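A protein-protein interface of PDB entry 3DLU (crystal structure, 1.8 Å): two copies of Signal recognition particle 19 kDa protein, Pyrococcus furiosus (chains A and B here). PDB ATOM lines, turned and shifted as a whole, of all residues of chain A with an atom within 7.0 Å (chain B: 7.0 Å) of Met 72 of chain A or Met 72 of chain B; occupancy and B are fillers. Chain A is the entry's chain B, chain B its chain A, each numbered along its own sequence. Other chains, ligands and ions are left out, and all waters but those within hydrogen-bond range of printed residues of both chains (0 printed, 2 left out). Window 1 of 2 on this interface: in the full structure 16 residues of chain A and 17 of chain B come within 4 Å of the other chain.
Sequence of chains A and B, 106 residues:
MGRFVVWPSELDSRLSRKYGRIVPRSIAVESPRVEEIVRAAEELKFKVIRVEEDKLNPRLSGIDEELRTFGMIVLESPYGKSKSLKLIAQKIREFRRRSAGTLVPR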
ATOM      1  N   VAL A   5     -20.537 -15.602 -10.849  1.00  0.00           N
ATOM      2  CA  VAL A   5     -20.873 -14.885  -9.629  1.00  0.00           C
ATOM      3  C   VAL A   5     -22.255 -14.260  -9.781  1.00  0.00           C
ATOM      4  O   VAL A   5     -22.641 -13.849 -10.872  1.00  0.00           O
ATOM      5  CB  VAL A   5     -19.793 -13.792  -9.279  1.00  0.00           C
ATOM      6  CG1 VAL A   5     -19.748 -12.695 -10.344  1.00  0.00           C
ATOM      7  CG2 VAL A   5     -20.036 -13.189  -7.902  1.00  0.00           C
ATOM      8  N   VAL A   6     -23.014 -14.256  -8.689  1.00  0.00           N
ATOM      9  CA  VAL A   6     -24.222 -13.446  -8.580  1.00  0.00           C
ATOM     10  C   VAL A   6     -23.980 -12.378  -7.514  1.00  0.00           C
ATOM     11  O   VAL A   6     -23.647 -12.682  -6.364  1.00  0.00           O
ATOM     12  CB  VAL A   6     -25.459 -14.287  -8.202  1.00  0.00           C
ATOM     13  CG1 VAL A   6     -26.670 -13.370  -7.935  1.00  0.00           C
ATOM     14  CG2 VAL A   6     -25.774 -15.314  -9.305  1.00  0.00           C
ATOM     15  N   TRP A   7     -24.134 -11.122  -7.916  1.00  0.00           N
ATOM     16  CA  TRP A   7     -24.029  -9.986  -7.003  1.00  0.00           C
ATOM     17  C   TRP A   7     -25.473  -9.504  -6.795  1.00  0.00           C
ATOM     18  O   TRP A   7     -26.176  -9.257  -7.758  1.00  0.00           O
ATOM     19  CB  TRP A   7     -23.133  -8.920  -7.661  1.00  0.00           C
ATOM     20  CG  TRP A   7     -22.988  -7.610  -6.920  1.00  0.00           C
ATOM     21  CD1 TRP A   7     -22.741  -7.434  -5.580  1.00  0.00           C
ATOM     22  CD2 TRP A   7     -23.061  -6.294  -7.488  1.00  0.00           C
ATOM     23  NE1 TRP A   7     -22.666  -6.086  -5.284  1.00  0.00           N
ATOM     24  CE2 TRP A   7     -22.866  -5.366  -6.432  1.00  0.00           C
ATOM     25  CE3 TRP A   7     -23.266  -5.807  -8.786  1.00  0.00           C
ATOM     26  CZ2 TRP A   7     -22.871  -3.985  -6.638  1.00  0.00           C
ATOM     27  CZ3 TRP A   7     -23.285  -4.427  -8.989  1.00  0.00           C
ATOM     28  CH2 TRP A   7     -23.088  -3.534  -7.918  1.00  0.00           C
ATOM     29  N   PRO A   8     -25.932  -9.394  -5.534  1.00  0.00           N
ATOM     30  CA  PRO A   8     -27.375  -9.200  -5.323  1.00  0.00           C
ATOM     31  C   PRO A   8     -27.938  -7.968  -6.024  1.00  0.00           C
ATOM     32  O   PRO A   8     -29.102  -7.980  -6.443  1.00  0.00           O
ATOM     33  CB  PRO A   8     -27.491  -9.061  -3.802  1.00  0.00           C
ATOM     34  CG  PRO A   8     -26.347  -9.857  -3.283  1.00  0.00           C
ATOM     35  CD  PRO A   8     -25.216  -9.594  -4.268  1.00  0.00           C
ATOM     36  N   VAL A  34     -28.908 -12.092   0.355  1.00  0.00           N
ATOM     37  CA  VAL A  34     -28.027 -13.197  -0.026  1.00  0.00           C
ATOM     38  C   VAL A  34     -28.676 -14.548   0.279  1.00  0.00           C
ATOM     39  O   VAL A  34     -28.656 -15.461  -0.544  1.00  0.00           O
ATOM     40  CB  VAL A  34     -26.645 -13.083   0.660  1.00  0.00           C
ATOM     41  CG1 VAL A  34     -25.865 -14.385   0.519  1.00  0.00           C
ATOM     42  CG2 VAL A  34     -25.848 -11.908   0.069  1.00  0.00           C
ATOM     43  N   VAL A  38     -29.506 -17.654  -2.222  1.00  0.00           N
ATOM     44  CA  VAL A  38     -29.075 -19.023  -1.940  1.00  0.00           C
ATOM     45  C   VAL A  38     -30.269 -19.984  -1.929  1.00  0.00           C
ATOM     46  O   VAL A  38     -30.214 -21.047  -2.539  1.00  0.00           O
ATOM     47  CB  VAL A  38     -28.301 -19.110  -0.616  1.00  0.00           C
ATOM     48  CG1 VAL A  38     -28.032 -20.564  -0.246  1.00  0.00           C
ATOM     49  CG2 VAL A  38     -26.992 -18.332  -0.722  1.00  0.00           C
ATOM     50  N   ARG A  50     -19.854 -20.773  -3.379  1.00  0.00           N
ATOM     51  CA  ARG A  50     -19.414 -19.883  -2.295  1.00  0.00           C
ATOM     52  C   ARG A  50     -20.498 -18.853  -1.974  1.00  0.00           C
ATOM     53  O   ARG A  50     -21.200 -18.383  -2.871  1.00  0.00           O
ATOM     54  CB  ARG A  50     -18.110 -19.165  -2.654  1.00  0.00           C
ATOM     55  CG  ARG A  50     -17.603 -18.221  -1.543  1.00  0.00           C
ATOM     56  CD  ARG A  50     -16.664 -17.117  -2.070  1.00  0.00           C
ATOM     57  NE  ARG A  50     -16.009 -16.384  -0.980  1.00  0.00           N
ATOM     58  CZ  ARG A  50     -15.648 -15.105  -1.037  1.00  0.00           C
ATOM     59  NH1 ARG A  50     -15.881 -14.386  -2.126  1.00  0.00           N
ATOM     60  NH2 ARG A  50     -15.056 -14.537   0.005  1.00  0.00           N
ATOM     61  N   VAL A  51     -20.623 -18.526  -0.693  1.00  0.00           N
ATOM     62  CA  VAL A  51     -21.548 -17.492  -0.236  1.00  0.00           C
ATOM     63  C   VAL A  51     -20.793 -16.581   0.721  1.00  0.00           C
ATOM     64  O   VAL A  51     -20.346 -17.036   1.774  1.00  0.00           O
ATOM     65  CB  VAL A  51     -22.728 -18.075   0.551  1.00  0.00           C
ATOM     66  CG1 VAL A  51     -23.688 -16.955   0.991  1.00  0.00           C
ATOM     67  CG2 VAL A  51     -23.481 -19.170  -0.252  1.00  0.00           C
ATOM     68  N   GLU A  52     -20.665 -15.305   0.370  1.00  0.00           N
ATOM     69  CA  GLU A  52     -20.008 -14.332   1.250  1.00  0.00           C
ATOM     70  C   GLU A  52     -20.983 -13.210   1.541  1.00  0.00           C
ATOM     71  O   GLU A  52     -21.619 -12.691   0.629  1.00  0.00           O
ATOM     72  CB  GLU A  52     -18.759 -13.735   0.594  1.00  0.00           C
ATOM     73  CG  GLU A  52     -17.810 -12.965   1.564  1.00  0.00           C
ATOM     74  CD  GLU A  52     -18.359 -11.632   2.126  1.00  0.00           C
ATOM     75  OE1 GLU A  52     -18.241 -11.406   3.356  1.00  0.00           O
ATOM     76  OE2 GLU A  52     -18.876 -10.796   1.356  1.00  0.00           O
ATOM     77  N   GLU A  53     -21.116 -12.843   2.809  1.00  0.00           N
ATOM     78  CA  GLU A  53     -21.977 -11.714   3.162  1.00  0.00           C
ATOM     79  C   GLU A  53     -21.422 -10.957   4.363  1.00  0.00           C
ATOM     80  O   GLU A  53     -20.844 -11.545   5.274  1.00  0.00           O
ATOM     81  CB  GLU A  53     -23.419 -12.160   3.407  1.00  0.00           C
ATOM     82  CG  GLU A  53     -23.584 -13.235   4.456  1.00  0.00           C
ATOM     83  CD  GLU A  53     -25.014 -13.767   4.525  1.00  0.00           C
ATOM     84  OE1 GLU A  53     -25.962 -12.940   4.555  1.00  0.00           O
ATOM     85  OE2 GLU A  53     -25.183 -15.012   4.546  1.00  0.00           O
ATOM     86  N   ASP A  54     -21.591  -9.642   4.336  1.00  0.00           N
ATOM     87  CA  ASP A  54     -21.072  -8.767   5.368  1.00  0.00           C
ATOM     88  C   ASP A  54     -22.210  -7.810   5.679  1.00  0.00           C
ATOM     89  O   ASP A  54     -22.745  -7.165   4.777  1.00  0.00           O
ATOM     90  CB  ASP A  54     -19.845  -8.008   4.845  1.00  0.00           C
ATOM     91  CG  ASP A  54     -19.021  -7.386   5.961  1.00  0.00           C
ATOM     92  OD1 ASP A  54     -19.384  -7.575   7.138  1.00  0.00           O
ATOM     93  OD2 ASP A  54     -18.001  -6.715   5.668  1.00  0.00           O
ATOM     94  N   PHE A  70     -23.894  -6.600   2.274  1.00  0.00           N
ATOM     95  CA  PHE A  70     -23.000  -6.683   1.130  1.00  0.00           C
ATOM     96  C   PHE A  70     -22.640  -8.152   0.925  1.00  0.00           C
ATOM     97  O   PHE A  70     -22.502  -8.898   1.892  1.00  0.00           O
ATOM     98  CB  PHE A  70     -21.732  -5.878   1.410  1.00  0.00           C
ATOM     99  CG  PHE A  70     -22.006  -4.458   1.823  1.00  0.00           C
ATOM    100  CD1 PHE A  70     -22.265  -4.143   3.152  1.00  0.00           C
ATOM    101  CD2 PHE A  70     -22.023  -3.444   0.883  1.00  0.00           C
ATOM    102  CE1 PHE A  70     -22.528  -2.839   3.530  1.00  0.00           C
ATOM    103  CE2 PHE A  70     -22.283  -2.137   1.259  1.00  0.00           C
ATOM    104  CZ  PHE A  70     -22.536  -1.836   2.581  1.00  0.00           C
ATOM    105  N   GLY A  71     -22.503  -8.586  -0.317  1.00  0.00           N
ATOM    106  CA  GLY A  71     -22.109  -9.962  -0.512  1.00  0.00           C
ATOM    107  C   GLY A  71     -22.083 -10.428  -1.946  1.00  0.00           C
ATOM    108  O   GLY A  71     -22.262  -9.647  -2.879  1.00  0.00           O
ATOM    109  N   MET A  72     -21.859 -11.722  -2.109  1.00  0.00           N
ATOM    110  CA  MET A  72     -21.741 -12.311  -3.434  1.00  0.00           C
ATOM    111  C   MET A  72     -21.957 -13.803  -3.268  1.00  0.00           C
ATOM    112  O   MET A  72     -21.696 -14.359  -2.191  1.00  0.00           O
ATOM    113  CB  MET A  72     -20.356 -12.032  -4.043  1.00  0.00           C
ATOM    114  CG  MET A  72     -19.187 -12.726  -3.344  1.00  0.00           C
ATOM    115  SD  MET A  72     -18.734 -14.356  -4.024  1.00  0.00           S
ATOM    116  CE  MET A  72     -17.501 -13.915  -5.256  1.00  0.00           C
ATOM    117  N   ILE A  73     -22.470 -14.430  -4.324  1.00  0.00           N
ATOM    118  CA  ILE A  73     -22.701 -15.872  -4.346  1.00  0.00           C
ATOM    119  C   ILE A  73     -22.042 -16.418  -5.613  1.00  0.00           C
ATOM    120  O   ILE A  73     -22.249 -15.875  -6.699  1.00  0.00           O
ATOM    121  CB  ILE A  73     -24.205 -16.192  -4.416  1.00  0.00           C
ATOM    122  CG1 ILE A  73     -24.957 -15.611  -3.206  1.00  0.00           C
ATOM    123  CG2 ILE A  73     -24.454 -17.687  -4.457  1.00  0.00           C
ATOM    124  CD1 ILE A  73     -25.466 -14.186  -3.415  1.00  0.00           C
ATOM    125  N   VAL A  74     -21.239 -17.470  -5.478  1.00  0.00           N
ATOM    126  CA  VAL A  74     -20.739 -18.178  -6.654  1.00  0.00           C
ATOM    127  C   VAL A  74     -21.605 -19.414  -6.856  1.00  0.00           C
ATOM    128  O   VAL A  74     -21.789 -20.206  -5.918  1.00  0.00           O
ATOM    129  CB  VAL A  74     -19.254 -18.593  -6.522  1.00  0.00           C
ATOM    130  CG1 VAL A  74     -18.817 -19.357  -7.780  1.00  0.00           C
ATOM    131  CG2 VAL A  74     -18.362 -17.348  -6.288  1.00  0.00           C
ATOM    132  N   VAL B   5     -19.756  -6.182 -10.779  1.00  0.00           N
ATOM    133  CA  VAL B   5     -18.837  -6.968  -9.986  1.00  0.00           C
ATOM    134  C   VAL B   5     -17.745  -7.571 -10.876  1.00  0.00           C
ATOM    135  O   VAL B   5     -17.994  -7.935 -12.023  1.00  0.00           O
ATOM    136  CB  VAL B   5     -19.583  -8.094  -9.225  1.00  0.00           C
ATOM    137  CG1 VAL B   5     -20.237  -9.076 -10.203  1.00  0.00           C
ATOM    138  CG2 VAL B   5     -18.644  -8.818  -8.278  1.00  0.00           C
ATOM    139  N   VAL B   6     -16.533  -7.630 -10.342  1.00  0.00           N
ATOM    140  CA  VAL B   6     -15.457  -8.418 -10.936  1.00  0.00           C
ATOM    141  C   VAL B   6     -15.100  -9.547  -9.979  1.00  0.00           C
ATOM    142  O   VAL B   6     -14.771  -9.328  -8.808  1.00  0.00           O
ATOM    143  CB  VAL B   6     -14.222  -7.567 -11.255  1.00  0.00           C
ATOM    144  CG1 VAL B   6     -13.086  -8.447 -11.817  1.00  0.00           C
ATOM    145  CG2 VAL B   6     -14.582  -6.459 -12.254  1.00  0.00           C
ATOM    146  N   TRP B   7     -15.201 -10.769 -10.476  1.00  0.00           N
ATOM    147  CA  TRP B   7     -14.839 -11.942  -9.708  1.00  0.00           C
ATOM    148  C   TRP B   7     -13.521 -12.442 -10.339  1.00  0.00           C
ATOM    149  O   TRP B   7     -13.468 -12.669 -11.550  1.00  0.00           O
ATOM    150  CB  TRP B   7     -15.997 -12.957  -9.797  1.00  0.00           C
ATOM    151  CG  TRP B   7     -15.717 -14.293  -9.187  1.00  0.00           C
ATOM    152  CD1 TRP B   7     -15.211 -14.538  -7.943  1.00  0.00           C
ATOM    153  CD2 TRP B   7     -15.970 -15.574  -9.780  1.00  0.00           C
ATOM    154  NE1 TRP B   7     -15.105 -15.902  -7.735  1.00  0.00           N
ATOM    155  CE2 TRP B   7     -15.569 -16.555  -8.848  1.00  0.00           C
ATOM    156  CE3 TRP B   7     -16.487 -15.986 -11.012  1.00  0.00           C
ATOM    157  CZ2 TRP B   7     -15.672 -17.929  -9.111  1.00  0.00           C
ATOM    158  CZ3 TRP B   7     -16.588 -17.355 -11.273  1.00  0.00           C
ATOM    159  CH2 TRP B   7     -16.177 -18.303 -10.322  1.00  0.00           C
ATOM    160  N   PRO B   8     -12.436 -12.527  -9.547  1.00  0.00           N
ATOM    161  CA  PRO B   8     -11.110 -12.774 -10.142  1.00  0.00           C
ATOM    162  C   PRO B   8     -11.076 -13.982 -11.090  1.00  0.00           C
ATOM    163  O   PRO B   8     -10.348 -13.962 -12.083  1.00  0.00           O
ATOM    164  CB  PRO B   8     -10.226 -13.020  -8.914  1.00  0.00           C
ATOM    165  CG  PRO B   8     -10.863 -12.158  -7.847  1.00  0.00           C
ATOM    166  CD  PRO B   8     -12.349 -12.360  -8.083  1.00  0.00           C
ATOM    167  N   VAL B  34      -6.861 -10.210  -5.960  1.00  0.00           N
ATOM    168  CA  VAL B  34      -7.787  -9.101  -5.751  1.00  0.00           C
ATOM    169  C   VAL B  34      -7.053  -7.758  -5.784  1.00  0.00           C
ATOM    170  O   VAL B  34      -7.528  -6.803  -6.407  1.00  0.00           O
ATOM    171  CB  VAL B  34      -8.557  -9.251  -4.420  1.00  0.00           C
ATOM    172  CG1 VAL B  34      -9.254  -7.942  -4.063  1.00  0.00           C
ATOM    173  CG2 VAL B  34      -9.565 -10.394  -4.517  1.00  0.00           C
ATOM    174  N   VAL B  38      -7.496  -4.469  -8.220  1.00  0.00           N
ATOM    175  CA  VAL B  38      -7.738  -3.126  -7.714  1.00  0.00           C
ATOM    176  C   VAL B  38      -6.700  -2.158  -8.287  1.00  0.00           C
ATOM    177  O   VAL B  38      -7.040  -1.068  -8.753  1.00  0.00           O
ATOM    178  CB  VAL B  38      -7.729  -3.078  -6.179  1.00  0.00           C
ATOM    179  CG1 VAL B  38      -7.670  -1.626  -5.685  1.00  0.00           C
ATOM    180  CG2 VAL B  38      -8.953  -3.793  -5.622  1.00  0.00           C
ATOM    181  N   ARG B  50     -16.307  -1.417  -3.878  1.00  0.00           N
ATOM    182  CA  ARG B  50     -16.137  -2.387  -2.785  1.00  0.00           C
ATOM    183  C   ARG B  50     -15.020  -3.367  -3.113  1.00  0.00           C
ATOM    184  O   ARG B  50     -14.897  -3.800  -4.249  1.00  0.00           O
ATOM    185  CB  ARG B  50     -17.418  -3.200  -2.547  1.00  0.00           C
ATOM    186  CG  ARG B  50     -17.203  -4.367  -1.547  1.00  0.00           C
ATOM    187  CD  ARG B  50     -18.484  -5.151  -1.242  1.00  0.00           C
ATOM    188  NE  ARG B  50     -18.356  -5.994  -0.046  1.00  0.00           N
ATOM    189  CZ  ARG B  50     -18.576  -7.308  -0.013  1.00  0.00           C
ATOM    190  NH1 ARG B  50     -18.929  -7.960  -1.113  1.00  0.00           N
ATOM    191  NH2 ARG B  50     -18.453  -7.978   1.131  1.00  0.00           N
ATOM    192  N   VAL B  51     -14.222  -3.727  -2.118  1.00  0.00           N
ATOM    193  CA  VAL B  51     -13.234  -4.793  -2.280  1.00  0.00           C
ATOM    194  C   VAL B  51     -13.380  -5.765  -1.129  1.00  0.00           C
ATOM    195  O   VAL B  51     -13.279  -5.367   0.019  1.00  0.00           O
ATOM    196  CB  VAL B  51     -11.797  -4.241  -2.242  1.00  0.00           C
ATOM    197  CG1 VAL B  51     -10.777  -5.357  -2.520  1.00  0.00           C
ATOM    198  CG2 VAL B  51     -11.637  -3.111  -3.229  1.00  0.00           C
ATOM    199  N   GLU B  52     -13.622  -7.039  -1.412  1.00  0.00           N
ATOM    200  CA  GLU B  52     -13.669  -8.017  -0.332  1.00  0.00           C
ATOM    201  C   GLU B  52     -12.691  -9.116  -0.654  1.00  0.00           C
ATOM    202  O   GLU B  52     -12.607  -9.555  -1.800  1.00  0.00           O
ATOM    203  CB  GLU B  52     -15.065  -8.625  -0.167  1.00  0.00           C
ATOM    204  CG  GLU B  52     -15.262  -9.379   1.162  1.00  0.00           C
ATOM    205  CD  GLU B  52     -14.695 -10.794   1.160  1.00  0.00           C
ATOM    206  OE1 GLU B  52     -14.628 -11.410   0.081  1.00  0.00           O
ATOM    207  OE2 GLU B  52     -14.329 -11.296   2.247  1.00  0.00           O
ATOM    208  N   GLU B  53     -11.958  -9.557   0.358  1.00  0.00           N
ATOM    209  CA  GLU B  53     -11.038 -10.673   0.179  1.00  0.00           C
ATOM    210  C   GLU B  53     -10.965 -11.529   1.442  1.00  0.00           C
ATOM    211  O   GLU B  53     -10.910 -11.015   2.557  1.00  0.00           O
ATOM    212  CB  GLU B  53      -9.654 -10.153  -0.207  1.00  0.00           C
ATOM    213  CG  GLU B  53      -8.735 -11.234  -0.733  1.00  0.00           C
ATOM    214  CD  GLU B  53      -7.358 -10.707  -1.081  1.00  0.00           C
ATOM    215  OE1 GLU B  53      -7.040  -9.565  -0.682  1.00  0.00           O
ATOM    216  OE2 GLU B  53      -6.600 -11.441  -1.749  1.00  0.00           O
ATOM    217  N   ASP B  54     -10.972 -12.843   1.262  1.00  0.00           N
ATOM    218  CA  ASP B  54     -10.887 -13.764   2.384  1.00  0.00           C
ATOM    219  C   ASP B  54      -9.729 -14.689   2.051  1.00  0.00           C
ATOM    220  O   ASP B  54      -9.682 -15.245   0.966  1.00  0.00           O
ATOM    221  CB  ASP B  54     -12.182 -14.568   2.517  1.00  0.00           C
ATOM    222  CG  ASP B  54     -12.273 -15.330   3.824  1.00  0.00           C
ATOM    223  OD1 ASP B  54     -11.380 -15.167   4.677  1.00  0.00           O
ATOM    224  OD2 ASP B  54     -13.251 -16.086   4.014  1.00  0.00           O
ATOM    225  N   PHE B  70     -10.078 -15.769  -1.783  1.00  0.00           N
ATOM    226  CA  PHE B  70     -11.409 -15.703  -2.370  1.00  0.00           C
ATOM    227  C   PHE B  70     -11.819 -14.249  -2.291  1.00  0.00           C
ATOM    228  O   PHE B  70     -11.510 -13.592  -1.308  1.00  0.00           O
ATOM    229  CB  PHE B  70     -12.363 -16.549  -1.538  1.00  0.00           C
ATOM    230  CG  PHE B  70     -11.891 -17.951  -1.334  1.00  0.00           C
ATOM    231  CD1 PHE B  70     -10.959 -18.247  -0.352  1.00  0.00           C
ATOM    232  CD2 PHE B  70     -12.358 -18.974  -2.145  1.00  0.00           C
ATOM    233  CE1 PHE B  70     -10.520 -19.535  -0.171  1.00  0.00           C
ATOM    234  CE2 PHE B  70     -11.921 -20.268  -1.966  1.00  0.00           C
ATOM    235  CZ  PHE B  70     -11.000 -20.550  -0.981  1.00  0.00           C
ATOM    236  N   GLY B  71     -12.483 -13.724  -3.310  1.00  0.00           N
ATOM    237  CA  GLY B  71     -12.788 -12.304  -3.271  1.00  0.00           C
ATOM    238  C   GLY B  71     -13.659 -11.788  -4.389  1.00  0.00           C
ATOM    239  O   GLY B  71     -14.084 -12.543  -5.272  1.00  0.00           O
ATOM    240  N   MET B  72     -13.933 -10.489  -4.338  1.00  0.00           N
ATOM    241  CA  MET B  72     -14.715  -9.816  -5.368  1.00  0.00           C
ATOM    242  C   MET B  72     -14.496  -8.326  -5.270  1.00  0.00           C
ATOM    243  O   MET B  72     -14.118  -7.805  -4.211  1.00  0.00           O
ATOM    244  CB  MET B  72     -16.215 -10.128  -5.247  1.00  0.00           C
ATOM    245  CG  MET B  72     -16.896  -9.522  -4.006  1.00  0.00           C
ATOM    246  SD  MET B  72     -17.594  -7.858  -4.209  1.00  0.00           S
ATOM    247  CE  MET B  72     -19.343  -8.227  -4.564  1.00  0.00           C
ATOM    248  N   ILE B  73     -14.704  -7.645  -6.383  1.00  0.00           N
ATOM    249  CA  ILE B  73     -14.507  -6.204  -6.447  1.00  0.00           C
ATOM    250  C   ILE B  73     -15.726  -5.633  -7.130  1.00  0.00           C
ATOM    251  O   ILE B  73     -16.172  -6.160  -8.144  1.00  0.00           O
ATOM    252  CB  ILE B  73     -13.258  -5.807  -7.288  1.00  0.00           C
ATOM    253  CG1 ILE B  73     -11.981  -6.500  -6.790  1.00  0.00           C
ATOM    254  CG2 ILE B  73     -13.069  -4.296  -7.261  1.00  0.00           C
ATOM    255  CD1 ILE B  73     -11.738  -7.884  -7.376  1.00  0.00           C
ATOM    256  N   VAL B  74     -16.286  -4.568  -6.570  1.00  0.00           N
ATOM    257  CA  VAL B  74     -17.315  -3.821  -7.263  1.00  0.00           C
ATOM    258  C   VAL B  74     -16.635  -2.583  -7.821  1.00  0.00           C
ATOM    259  O   VAL B  74     -15.936  -1.876  -7.097  1.00  0.00           O
ATOM    260  CB  VAL B  74     -18.450  -3.402  -6.302  1.00  0.00           C
ATOM    261  CG1 VAL B  74     -19.467  -2.564  -7.045  1.00  0.00           C
ATOM    262  CG2 VAL B  74     -19.114  -4.649  -5.690  1.00  0.00           C
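Of the printed residues of chain B, Trp 7 of chain A touches Val 5, Met 72 and Val 74.
Val 34 of chain A touches none of the printed residues of chain B.
Of chain B, only Trp 7, Gly 71 and Met 72 come within 4 Å of Met 72 of chain A.
Of the printed residues of chain A, Phe 70 of chain B touches Arg 50 (3.6 Å).
Of the printed residues of chain A, Gly 71 of chain B touches Arg 50 (3.7 Å) and Met 72 (3.7 Å).
The nearest residue of chain B that does not touch Met 72 of chain A is Arg 50 of chain B (4.9 Å).
The nearest residue of chain A that does not touch Met 72 of chain B is Arg 50 of chain A (4.9 Å).
Among the printed residues, pairs that only touch across the chains: Met 72 of chain A with Trp 7 of chain B, Arg 50 of chain A with Phe 70 of chain B, Trp 7 of chain A with Met 72 of chain B, Val 5 of chain A with Val 5 of chain B, Gly 71 of chain A with Met 72 of chain B, Arg 50 of chain A with Gly 71 of chain B, Phe 70 of chain A with Arg 50 of chain B, Met 72 of chain A with Gly 71 of chain B, Val 74 of chain A with Trp 7 of chain B, Trp 7 of chain A with Val 74 of chain B, Gly 71 of chain A with Arg 50 of chain B, Val 5 of chain A with Trp 7 of chain B, Arg 50 of chain A with Asp 54 of chain B, Glu 52 of chain A with Glu 52 of chain B, Trp 7 of chain A with Val 5 of chain B, Asp 54 of chain A with Arg 50 of chain B and Met 72 of chain A with Met 72 of chain B.
Trp 7 of chain A touches Met 72 of chain B, and with the chains exchanged Met 72 of chain A touches Trp 7 of chain B.
Trp 7 of chain A touches Val 74 of chain B, and with the chains exchanged Val 74 of chain A touches Trp 7 of chain B.
Arg 50 of chain A touches Phe 70 of chain B, and with the chains exchanged Phe 70 of chain A touches Arg 50 of chain B.
Arg 50 of chain A touches Gly 71 of chain B, and with the chains exchanged Gly 71 of chain A touches Arg 50 of chain B.
Positions printed for both chains: 5, 6, 7, 8, 34, 38, 50, 51, 52, 53, 54, 70, 71, 72, 73 and 74.
The backbone NH (N) of Val 74 of chain A is in hydrogen-bond range of the backbone carbonyl oxygen (O) of Arg 50 of chain A (2.8 Å).
The guanidinium group (NH1) of Arg 50 of chain A sits at hydrogen-bond distance from the side-chain sulfur (SD) of Met 72 of chain A, 3.4 Å away.
O of Met 72 of chain B lies within hydrogen-bond range of N of Glu 52 of chain B (2.9 Å).
O of Phe 70 of chain B sits at hydrogen-bond distance from N of Asp 54 of chain B (2.7 Å).
NH1 of Arg 50 of chain B lies within hydrogen-bond range of SD of Met 72 of chain B (3.4 Å).
The backbone NH of Asp 54 of chain A sits at hydrogen-bond distance from the backbone carbonyl oxygen of Phe 70 of chain A, at 2.7 Å.
Of the 16 printed residues of chain A, 9 touch a printed residue of chain B.
Hydrophobic or aromatic side chains of chain A within 4 Å of the printed part of chain B: Val 5, Trp 7, Phe 70, Met 72 and Val 74.
Of the 16 printed residues of chain B, 9 touch a printed residue of chain A.
Hydrophobic or aromatic side chains of chain B that line the printed part of chain A: Val 5, Trp 7, Phe 70, Met 72 and Val 74.
Along chain B the printed residues that touch a printed residue of chain A span positions 5 to 74.
Among the printed residues, Asp or Glu carboxylates within 4 Å of a Lys or Arg side-chain nitrogen of the other chain: Arg 50 of chain A with Glu 52 of chain B (3.2 Å) and Glu 52 of chain A with Arg 50 of chain B (2.9 Å).
NH2 of Arg 50 of chain B lies within salt-bridge range of OE2 of Glu 52 of chain A, at 2.9 Å.
The side-chain carboxylate (OE1) of Glu 52 of chain B is in salt-bridge range of the guanidinium group (NH2) of Arg 50 of chain A (3.2 Å).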
